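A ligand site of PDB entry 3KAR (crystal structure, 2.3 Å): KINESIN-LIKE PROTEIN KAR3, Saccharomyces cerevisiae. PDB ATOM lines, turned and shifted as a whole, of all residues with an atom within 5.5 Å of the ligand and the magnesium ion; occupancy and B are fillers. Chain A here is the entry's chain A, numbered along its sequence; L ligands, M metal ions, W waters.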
ATOM      1  N   ARG A   9     -30.986 -29.223 -28.655  1.00  0.00           N
ATOM      2  CA  ARG A   9     -31.291 -28.352 -27.572  1.00  0.00           C
ATOM      3  C   ARG A   9     -30.563 -27.040 -27.719  1.00  0.00           C
ATOM      4  O   ARG A   9     -29.339 -26.971 -27.867  1.00  0.00           O
ATOM      5  CB  ARG A   9     -31.083 -29.039 -26.211  1.00  0.00           C
ATOM      6  CG  ARG A   9     -31.472 -28.253 -24.954  1.00  0.00           C
ATOM      7  CD  ARG A   9     -30.418 -28.487 -23.900  1.00  0.00           C
ATOM      8  NE  ARG A   9     -30.817 -28.542 -22.486  1.00  0.00           N
ATOM      9  CZ  ARG A   9     -31.367 -27.593 -21.825  1.00  0.00           C
ATOM     10  NH1 ARG A   9     -31.782 -26.513 -22.427  1.00  0.00           N
ATOM     11  NH2 ARG A   9     -31.572 -27.748 -20.538  1.00  0.00           N
ATOM     12  N   ILE A  10     -31.333 -25.980 -27.700  1.00  0.00           N
ATOM     13  CA  ILE A  10     -30.734 -24.653 -27.812  1.00  0.00           C
ATOM     14  C   ILE A  10     -30.635 -24.037 -26.450  1.00  0.00           C
ATOM     15  O   ILE A  10     -31.616 -23.891 -25.723  1.00  0.00           O
ATOM     16  CB  ILE A  10     -31.527 -23.714 -28.720  1.00  0.00           C
ATOM     17  CG1 ILE A  10     -31.922 -24.391 -30.032  1.00  0.00           C
ATOM     18  CG2 ILE A  10     -30.762 -22.419 -28.946  1.00  0.00           C
ATOM     19  CD1 ILE A  10     -32.813 -23.537 -30.933  1.00  0.00           C
ATOM     20  N   ARG A  11     -29.452 -23.715 -26.065  1.00  0.00           N
ATOM     21  CA  ARG A  11     -29.306 -23.136 -24.777  1.00  0.00           C
ATOM     22  C   ARG A  11     -29.494 -21.617 -24.797  1.00  0.00           C
ATOM     23  O   ARG A  11     -29.351 -20.915 -25.807  1.00  0.00           O
ATOM     24  CB  ARG A  11     -27.926 -23.496 -24.230  1.00  0.00           C
ATOM     25  CG  ARG A  11     -26.750 -22.840 -24.959  1.00  0.00           C
ATOM     26  CD  ARG A  11     -25.567 -22.585 -24.003  1.00  0.00           C
ATOM     27  NE  ARG A  11     -24.327 -22.183 -24.665  1.00  0.00           N
ATOM     28  CZ  ARG A  11     -24.080 -20.940 -25.058  1.00  0.00           C
ATOM     29  NH1 ARG A  11     -24.949 -19.951 -24.919  1.00  0.00           N
ATOM     30  NH2 ARG A  11     -22.929 -20.679 -25.609  1.00  0.00           N
ATOM     31  N   PRO A  12     -29.774 -21.083 -23.654  1.00  0.00           N
ATOM     32  CA  PRO A  12     -29.903 -19.675 -23.607  1.00  0.00           C
ATOM     33  C   PRO A  12     -28.551 -19.010 -23.857  1.00  0.00           C
ATOM     34  O   PRO A  12     -27.479 -19.581 -23.629  1.00  0.00           O
ATOM     35  CB  PRO A  12     -30.461 -19.326 -22.226  1.00  0.00           C
ATOM     36  CG  PRO A  12     -30.657 -20.632 -21.489  1.00  0.00           C
ATOM     37  CD  PRO A  12     -30.027 -21.707 -22.350  1.00  0.00           C
ATOM     38  N   LEU A  14     -25.377 -16.286 -23.675  1.00  0.00           N
ATOM     39  CA  LEU A  14     -24.607 -15.759 -22.587  1.00  0.00           C
ATOM     40  C   LEU A  14     -24.741 -14.236 -22.484  1.00  0.00           C
ATOM     41  O   LEU A  14     -24.489 -13.509 -23.435  1.00  0.00           O
ATOM     42  CB  LEU A  14     -23.128 -16.169 -22.661  1.00  0.00           C
ATOM     43  CG  LEU A  14     -22.779 -17.481 -21.928  1.00  0.00           C
ATOM     44  CD1 LEU A  14     -23.911 -18.508 -22.010  1.00  0.00           C
ATOM     45  CD2 LEU A  14     -21.533 -18.064 -22.558  1.00  0.00           C
ATOM     46  N   ASP A  63     -37.165 -24.226 -22.348  1.00  0.00           N
ATOM     47  CA  ASP A  63     -37.072 -25.551 -21.738  1.00  0.00           C
ATOM     48  C   ASP A  63     -35.901 -25.667 -20.775  1.00  0.00           C
ATOM     49  O   ASP A  63     -34.766 -25.542 -21.201  1.00  0.00           O
ATOM     50  CB  ASP A  63     -36.878 -26.595 -22.826  1.00  0.00           C
ATOM     51  CG  ASP A  63     -38.005 -26.574 -23.800  1.00  0.00           C
ATOM     52  OD1 ASP A  63     -39.149 -26.438 -23.443  1.00  0.00           O
ATOM     53  OD2 ASP A  63     -37.620 -26.703 -25.043  1.00  0.00           O
ATOM     54  N   ASN A  65     -33.853 -27.854 -17.560  1.00  0.00           N
ATOM     55  CA  ASN A  65     -33.456 -29.249 -17.376  1.00  0.00           C
ATOM     56  C   ASN A  65     -34.670 -30.099 -16.977  1.00  0.00           C
ATOM     57  O   ASN A  65     -34.967 -31.167 -17.570  1.00  0.00           O
ATOM     58  CB  ASN A  65     -32.286 -29.389 -16.367  1.00  0.00           C
ATOM     59  CG  ASN A  65     -30.930 -29.205 -17.043  1.00  0.00           C
ATOM     60  OD1 ASN A  65     -30.904 -29.036 -18.240  1.00  0.00           O
ATOM     61  ND2 ASN A  65     -29.819 -29.256 -16.287  1.00  0.00           N
ATOM     62  N   GLY A  91     -21.876 -32.049 -29.253  1.00  0.00           N
ATOM     63  CA  GLY A  91     -21.794 -30.643 -29.523  1.00  0.00           C
ATOM     64  C   GLY A  91     -20.471 -30.002 -29.202  1.00  0.00           C
ATOM     65  O   GLY A  91     -19.621 -30.580 -28.548  1.00  0.00           O
ATOM     66  N   GLN A  92     -20.330 -28.767 -29.655  1.00  0.00           N
ATOM     67  CA  GLN A  92     -19.117 -27.997 -29.491  1.00  0.00           C
ATOM     68  C   GLN A  92     -18.893 -27.584 -28.063  1.00  0.00           C
ATOM     69  O   GLN A  92     -19.859 -27.354 -27.301  1.00  0.00           O
ATOM     70  CB  GLN A  92     -19.159 -26.756 -30.406  1.00  0.00           C
ATOM     71  CG  GLN A  92     -19.849 -25.555 -29.733  1.00  0.00           C
ATOM     72  CD  GLN A  92     -19.765 -24.321 -30.623  1.00  0.00           C
ATOM     73  OE1 GLN A  92     -18.749 -23.628 -30.664  1.00  0.00           O
ATOM     74  NE2 GLN A  92     -20.805 -24.040 -31.369  1.00  0.00           N
ATOM     75  N   THR A  93     -17.621 -27.445 -27.707  1.00  0.00           N
ATOM     76  CA  THR A  93     -17.340 -26.962 -26.377  1.00  0.00           C
ATOM     77  C   THR A  93     -18.128 -25.691 -26.130  1.00  0.00           C
ATOM     78  O   THR A  93     -18.234 -24.797 -26.984  1.00  0.00           O
ATOM     79  CB  THR A  93     -15.847 -26.807 -26.036  1.00  0.00           C
ATOM     80  OG1 THR A  93     -15.193 -28.003 -26.346  1.00  0.00           O
ATOM     81  CG2 THR A  93     -15.699 -26.537 -24.553  1.00  0.00           C
ATOM     82  N   GLY A  94     -18.820 -25.680 -25.031  1.00  0.00           N
ATOM     83  CA  GLY A  94     -19.598 -24.568 -24.698  1.00  0.00           C
ATOM     84  C   GLY A  94     -21.067 -24.663 -25.094  1.00  0.00           C
ATOM     85  O   GLY A  94     -21.865 -23.798 -24.682  1.00  0.00           O
ATOM     86  N   SER A  95     -21.443 -25.644 -25.889  1.00  0.00           N
ATOM     87  CA  SER A  95     -22.850 -25.687 -26.287  1.00  0.00           C
ATOM     88  C   SER A  95     -23.816 -26.007 -25.160  1.00  0.00           C
ATOM     89  O   SER A  95     -25.021 -25.839 -25.330  1.00  0.00           O
ATOM     90  CB  SER A  95     -23.059 -26.588 -27.501  1.00  0.00           C
ATOM     91  OG  SER A  95     -22.404 -27.794 -27.257  1.00  0.00           O
ATOM     92  N   GLY A  96     -23.250 -26.533 -24.047  1.00  0.00           N
ATOM     93  CA  GLY A  96     -23.993 -26.971 -22.863  1.00  0.00           C
ATOM     94  C   GLY A  96     -24.119 -28.519 -22.713  1.00  0.00           C
ATOM     95  O   GLY A  96     -25.157 -29.036 -22.254  1.00  0.00           O
ATOM     96  N   LYS A  97     -23.100 -29.318 -23.068  1.00  0.00           N
ATOM     97  CA  LYS A  97     -23.294 -30.747 -22.938  1.00  0.00           C
ATOM     98  C   LYS A  97     -23.264 -31.231 -21.497  1.00  0.00           C
ATOM     99  O   LYS A  97     -24.052 -32.077 -21.054  1.00  0.00           O
ATOM    100  CB  LYS A  97     -22.376 -31.580 -23.796  1.00  0.00           C
ATOM    101  CG  LYS A  97     -22.139 -31.057 -25.180  1.00  0.00           C
ATOM    102  CD  LYS A  97     -21.199 -31.956 -25.959  1.00  0.00           C
ATOM    103  CE  LYS A  97     -19.755 -31.814 -25.512  1.00  0.00           C
ATOM    104  NZ  LYS A  97     -19.323 -30.427 -25.287  1.00  0.00           N
ATOM    105  N   THR A  98     -22.344 -30.720 -20.765  1.00  0.00           N
ATOM    106  CA  THR A  98     -22.208 -31.131 -19.370  1.00  0.00           C
ATOM    107  C   THR A  98     -23.374 -30.638 -18.517  1.00  0.00           C
ATOM    108  O   THR A  98     -23.792 -31.272 -17.537  1.00  0.00           O
ATOM    109  CB  THR A  98     -20.841 -30.639 -18.877  1.00  0.00           C
ATOM    110  OG1 THR A  98     -19.824 -31.364 -19.557  1.00  0.00           O
ATOM    111  CG2 THR A  98     -20.675 -30.757 -17.374  1.00  0.00           C
ATOM    112  N   PHE A  99     -23.917 -29.500 -18.921  1.00  0.00           N
ATOM    113  CA  PHE A  99     -24.998 -28.889 -18.214  1.00  0.00           C
ATOM    114  C   PHE A  99     -26.222 -29.782 -18.235  1.00  0.00           C
ATOM    115  O   PHE A  99     -26.904 -29.994 -17.232  1.00  0.00           O
ATOM    116  CB  PHE A  99     -25.282 -27.453 -18.736  1.00  0.00           C
ATOM    117  CG  PHE A  99     -26.432 -26.775 -17.994  1.00  0.00           C
ATOM    118  CD1 PHE A  99     -27.744 -26.960 -18.409  1.00  0.00           C
ATOM    119  CD2 PHE A  99     -26.198 -25.946 -16.890  1.00  0.00           C
ATOM    120  CE1 PHE A  99     -28.805 -26.335 -17.747  1.00  0.00           C
ATOM    121  CE2 PHE A  99     -27.241 -25.322 -16.211  1.00  0.00           C
ATOM    122  CZ  PHE A  99     -28.549 -25.495 -16.665  1.00  0.00           C
ATOM    123  N   THR A 100     -26.479 -30.270 -19.408  1.00  0.00           N
ATOM    124  CA  THR A 100     -27.588 -31.146 -19.767  1.00  0.00           C
ATOM    125  C   THR A 100     -27.437 -32.525 -19.061  1.00  0.00           C
ATOM    126  O   THR A 100     -28.426 -33.110 -18.586  1.00  0.00           O
ATOM    127  CB  THR A 100     -27.529 -31.287 -21.341  1.00  0.00           C
ATOM    128  OG1 THR A 100     -27.806 -30.064 -21.945  1.00  0.00           O
ATOM    129  CG2 THR A 100     -28.409 -32.338 -21.948  1.00  0.00           C
ATOM    130  N   ARG A 202     -15.591 -30.159 -14.396  1.00  0.00           N
ATOM    131  CA  ARG A 202     -15.964 -29.774 -15.739  1.00  0.00           C
ATOM    132  C   ARG A 202     -16.446 -28.338 -15.836  1.00  0.00           C
ATOM    133  O   ARG A 202     -16.898 -27.905 -16.878  1.00  0.00           O
ATOM    134  CB  ARG A 202     -16.966 -30.740 -16.354  1.00  0.00           C
ATOM    135  CG  ARG A 202     -16.401 -32.128 -16.392  1.00  0.00           C
ATOM    136  CD  ARG A 202     -17.388 -33.306 -16.725  1.00  0.00           C
ATOM    137  NE  ARG A 202     -16.951 -34.284 -15.739  1.00  0.00           N
ATOM    138  CZ  ARG A 202     -15.923 -35.116 -15.865  1.00  0.00           C
ATOM    139  NH1 ARG A 202     -15.310 -35.264 -17.058  1.00  0.00           N
ATOM    140  NH2 ARG A 202     -15.665 -35.900 -14.874  1.00  0.00           N
ATOM    141  N   ASN A 210     -11.311 -28.445 -17.390  1.00  0.00           N
ATOM    142  CA  ASN A 210     -12.071 -28.709 -18.600  1.00  0.00           C
ATOM    143  C   ASN A 210     -11.244 -28.900 -19.862  1.00  0.00           C
ATOM    144  O   ASN A 210     -11.710 -29.552 -20.801  1.00  0.00           O
ATOM    145  CB  ASN A 210     -13.350 -27.836 -18.765  1.00  0.00           C
ATOM    146  CG  ASN A 210     -14.444 -28.397 -19.683  1.00  0.00           C
ATOM    147  OD1 ASN A 210     -14.910 -27.697 -20.607  1.00  0.00           O
ATOM    148  ND2 ASN A 210     -14.882 -29.647 -19.435  1.00  0.00           N
ATOM    149  N   SER A 214     -12.953 -31.589 -22.131  1.00  0.00           N
ATOM    150  CA  SER A 214     -13.377 -31.061 -23.420  1.00  0.00           C
ATOM    151  C   SER A 214     -12.952 -31.993 -24.494  1.00  0.00           C
ATOM    152  O   SER A 214     -13.642 -32.181 -25.493  1.00  0.00           O
ATOM    153  CB  SER A 214     -12.560 -29.790 -23.699  1.00  0.00           C
ATOM    154  OG  SER A 214     -13.284 -28.739 -23.135  1.00  0.00           O
ATOM    155  N   ASP A 243     -21.256 -38.028 -22.227  1.00  0.00           N
ATOM    156  CA  ASP A 243     -20.836 -36.655 -22.326  1.00  0.00           C
ATOM    157  C   ASP A 243     -19.642 -36.637 -23.275  1.00  0.00           C
ATOM    158  O   ASP A 243     -18.467 -36.742 -22.851  1.00  0.00           O
ATOM    159  CB  ASP A 243     -20.515 -35.982 -20.981  1.00  0.00           C
ATOM    160  CG  ASP A 243     -20.202 -34.511 -21.146  1.00  0.00           C
ATOM    161  OD1 ASP A 243     -20.344 -33.899 -22.175  1.00  0.00           O
ATOM    162  OD2 ASP A 243     -19.737 -33.945 -20.077  1.00  0.00           O
HETATM  163  P1  LIG L   1     -20.054 -27.937 -22.716  1.00  0.00           P
HETATM  164  O1  LIG L   1     -20.834 -28.259 -23.983  1.00  0.00           O
HETATM  165  O2  LIG L   1     -20.124 -29.108 -21.766  1.00  0.00           O
HETATM  166  O3  LIG L   1     -18.550 -27.543 -23.018  1.00  0.00           O
HETATM  167  P2  LIG L   1     -21.283 -26.553 -20.623  1.00  0.00           P
HETATM  168  O4  LIG L   1     -22.160 -27.697 -20.195  1.00  0.00           O
HETATM  169  O5  LIG L   1     -20.099 -26.561 -19.729  1.00  0.00           O
HETATM  170  O6  LIG L   1     -20.759 -26.730 -22.068  1.00  0.00           O
HETATM  171  O7  LIG L   1     -22.154 -25.212 -20.576  1.00  0.00           O
HETATM  172  C1  LIG L   1     -21.510 -23.990 -20.982  1.00  0.00           C
HETATM  173  C2  LIG L   1     -22.118 -22.848 -20.162  1.00  0.00           C
HETATM  174  O8  LIG L   1     -23.519 -22.710 -20.571  1.00  0.00           O
HETATM  175  C3  LIG L   1     -22.138 -23.074 -18.642  1.00  0.00           C
HETATM  176  O9  LIG L   1     -21.754 -21.904 -17.890  1.00  0.00           O
HETATM  177  C4  LIG L   1     -23.577 -23.528 -18.418  1.00  0.00           C
HETATM  178  O10 LIG L   1     -23.973 -23.173 -17.100  1.00  0.00           O
HETATM  179  C5  LIG L   1     -24.381 -22.789 -19.477  1.00  0.00           C
HETATM  180  N1  LIG L   1     -25.498 -23.590 -19.964  1.00  0.00           N
HETATM  181  C6  LIG L   1     -25.439 -24.666 -20.774  1.00  0.00           C
HETATM  182  N2  LIG L   1     -26.634 -25.108 -21.141  1.00  0.00           N
HETATM  183  C7  LIG L   1     -27.509 -24.333 -20.391  1.00  0.00           C
HETATM  184  C8  LIG L   1     -28.903 -24.382 -20.322  1.00  0.00           C
HETATM  185  N3  LIG L   1     -29.652 -25.192 -20.918  1.00  0.00           N
HETATM  186  N4  LIG L   1     -29.354 -23.395 -19.518  1.00  0.00           N
HETATM  187  C9  LIG L   1     -28.617 -22.515 -18.810  1.00  0.00           C
HETATM  188  N5  LIG L   1     -27.332 -22.454 -18.872  1.00  0.00           N
HETATM  189  C10 LIG L   1     -26.836 -23.383 -19.703  1.00  0.00           C
HETATM  190 MG    MG M   1     -18.639 -30.305 -21.011  1.00  0.00          MG
HETATM  191  O   HOH W   1     -16.945 -29.851 -25.094  1.00  0.00           O
HETATM  192  O   HOH W   2     -25.058 -21.140 -16.299  1.00  0.00           O
HETATM  193  O   HOH W   3     -31.690 -23.821 -18.612  1.00  0.00           O
HETATM  194  O   HOH W   4     -18.246 -31.931 -22.130  1.00  0.00           O
HETATM  195  O   HOH W   5     -28.156 -26.659 -22.491  1.00  0.00           O
HETATM  196  O   HOH W   6     -17.324 -25.615 -21.736  1.00  0.00           O
HETATM  197  O   HOH W   7     -18.363 -28.796 -19.821  1.00  0.00           O
HETATM  198  O   HOH W   8     -16.916 -29.559 -21.802  1.00  0.00           O
HETATM  199  O   HOH W   9     -16.853 -30.978 -19.876  1.00  0.00           O
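N of Gly 94 lies within hydrogen-bond range of O3 of the ligand.
The backbone NH (N) of Ser 95 is in hydrogen-bond range of an oxygen (O1) of the ligand.
N of Thr 98 is in hydrogen-bond range of O4 of the ligand (3.1 Å).
N of Gly 96 sits at hydrogen-bond distance from O1 of the ligand, 3.0 Å away.
N of Phe 99 sits at hydrogen-bond distance from O4 of the ligand (2.8 Å).
O1 of the ligand lies within hydrogen-bond range of N of Lys 97, at 2.7 Å.
NZ of Lys 97 lies within salt-bridge range of O1 of the ligand (2.9 Å).
O of Phe 99 lies within hydrogen-bond range of ND2 of Asn 65 (3.2 Å).
The guanidinium group (NE) of Arg 11 sits at hydrogen-bond distance from the backbone carbonyl oxygen (O) of Gly 94 (2.9 Å).
NH1 of Arg 9 sits at hydrogen-bond distance from O of Asp 63 (3.4 Å).
The side-chain amino group (NZ) of Lys 97 lies within hydrogen-bond range of the backbone carbonyl oxygen (O) of Gly 91, 3.3 Å away.
The backbone carbonyl oxygen (O) of Gly 96 sits at hydrogen-bond distance from the side-chain hydroxyl (OG1) of Thr 100 (2.9 Å).
The guanidinium group (NE) of Arg 9 sits at hydrogen-bond distance from the side-chain hydroxyl (OG1) of Thr 100 (3.4 Å).
The side-chain hydroxyl (OG1) of Thr 98 sits close to the side-chain carboxylate (OD2) of Asp 243 (2.6 Å).
The guanidinium group (NH2) of Arg 9 sits at hydrogen-bond distance from the side-chain amide oxygen (OD1) of Asn 65, at 2.7 Å.
NH1 of Arg 9 lies close to N3 of the ligand (2.9 Å).
Residues that only touch the ligand: Pro 12 (3.4 Å), Thr 93 (3.4 Å), Gln 92 (3.6 Å) and Arg 11 (3.7 Å).
Hydrophobic or aromatic side chains that line the ligand: Pro 12 and Phe 99.
Of the 21 residues printed, 11 come within 4 Å of the ligand.
The nearest printed residue that does not touch the ligand is Asn 210 (4.4 Å).
Asp 243 touches the magnesium ion (OD2 to MG, 3.9 Å).
Of the 21 residues printed, 2 come within 4 Å of the magnesium ion.
The nearest printed residue that does not touch the magnesium ion is Asn 210 (4.1 Å).
Water W7 is bound to the magnesium ion.
Water W4 is bound to the magnesium ion (2.0 Å).
The magnesium ion is bound by water W8, at 2.0 Å.
The magnesium ion is bound by an oxygen (O2) of the ligand.
OG1 of Thr 98 is bound to the magnesium ion (2.2 Å).
Water W9 binds the magnesium ion (2.2 Å).
The magnesium ion has six donor atoms within binding distance.
Water W7 lies within hydrogen-bond range of O5 of the ligand and O of Arg 202.
Water W8 lies within hydrogen-bond range of an oxygen (O3) of the ligand (2.9 Å) and the side-chain amide oxygen of Asn 210 (3.0 Å).
Water W5 lies within hydrogen-bond range of N2 of the ligand (2.6 Å), NE of Arg 9 (3.3 Å) and OG1 of Thr 100 (3.5 Å).
Water W6 lies within hydrogen-bond range of O3 of the ligand (2.6 Å) and OD1 of Asn 210 (3.4 Å).
Water W1 lies within hydrogen-bond range of NZ of Lys 97 (2.5 Å), OG1 of Thr 93 (2.8 Å) and O3 of the ligand (3.5 Å).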
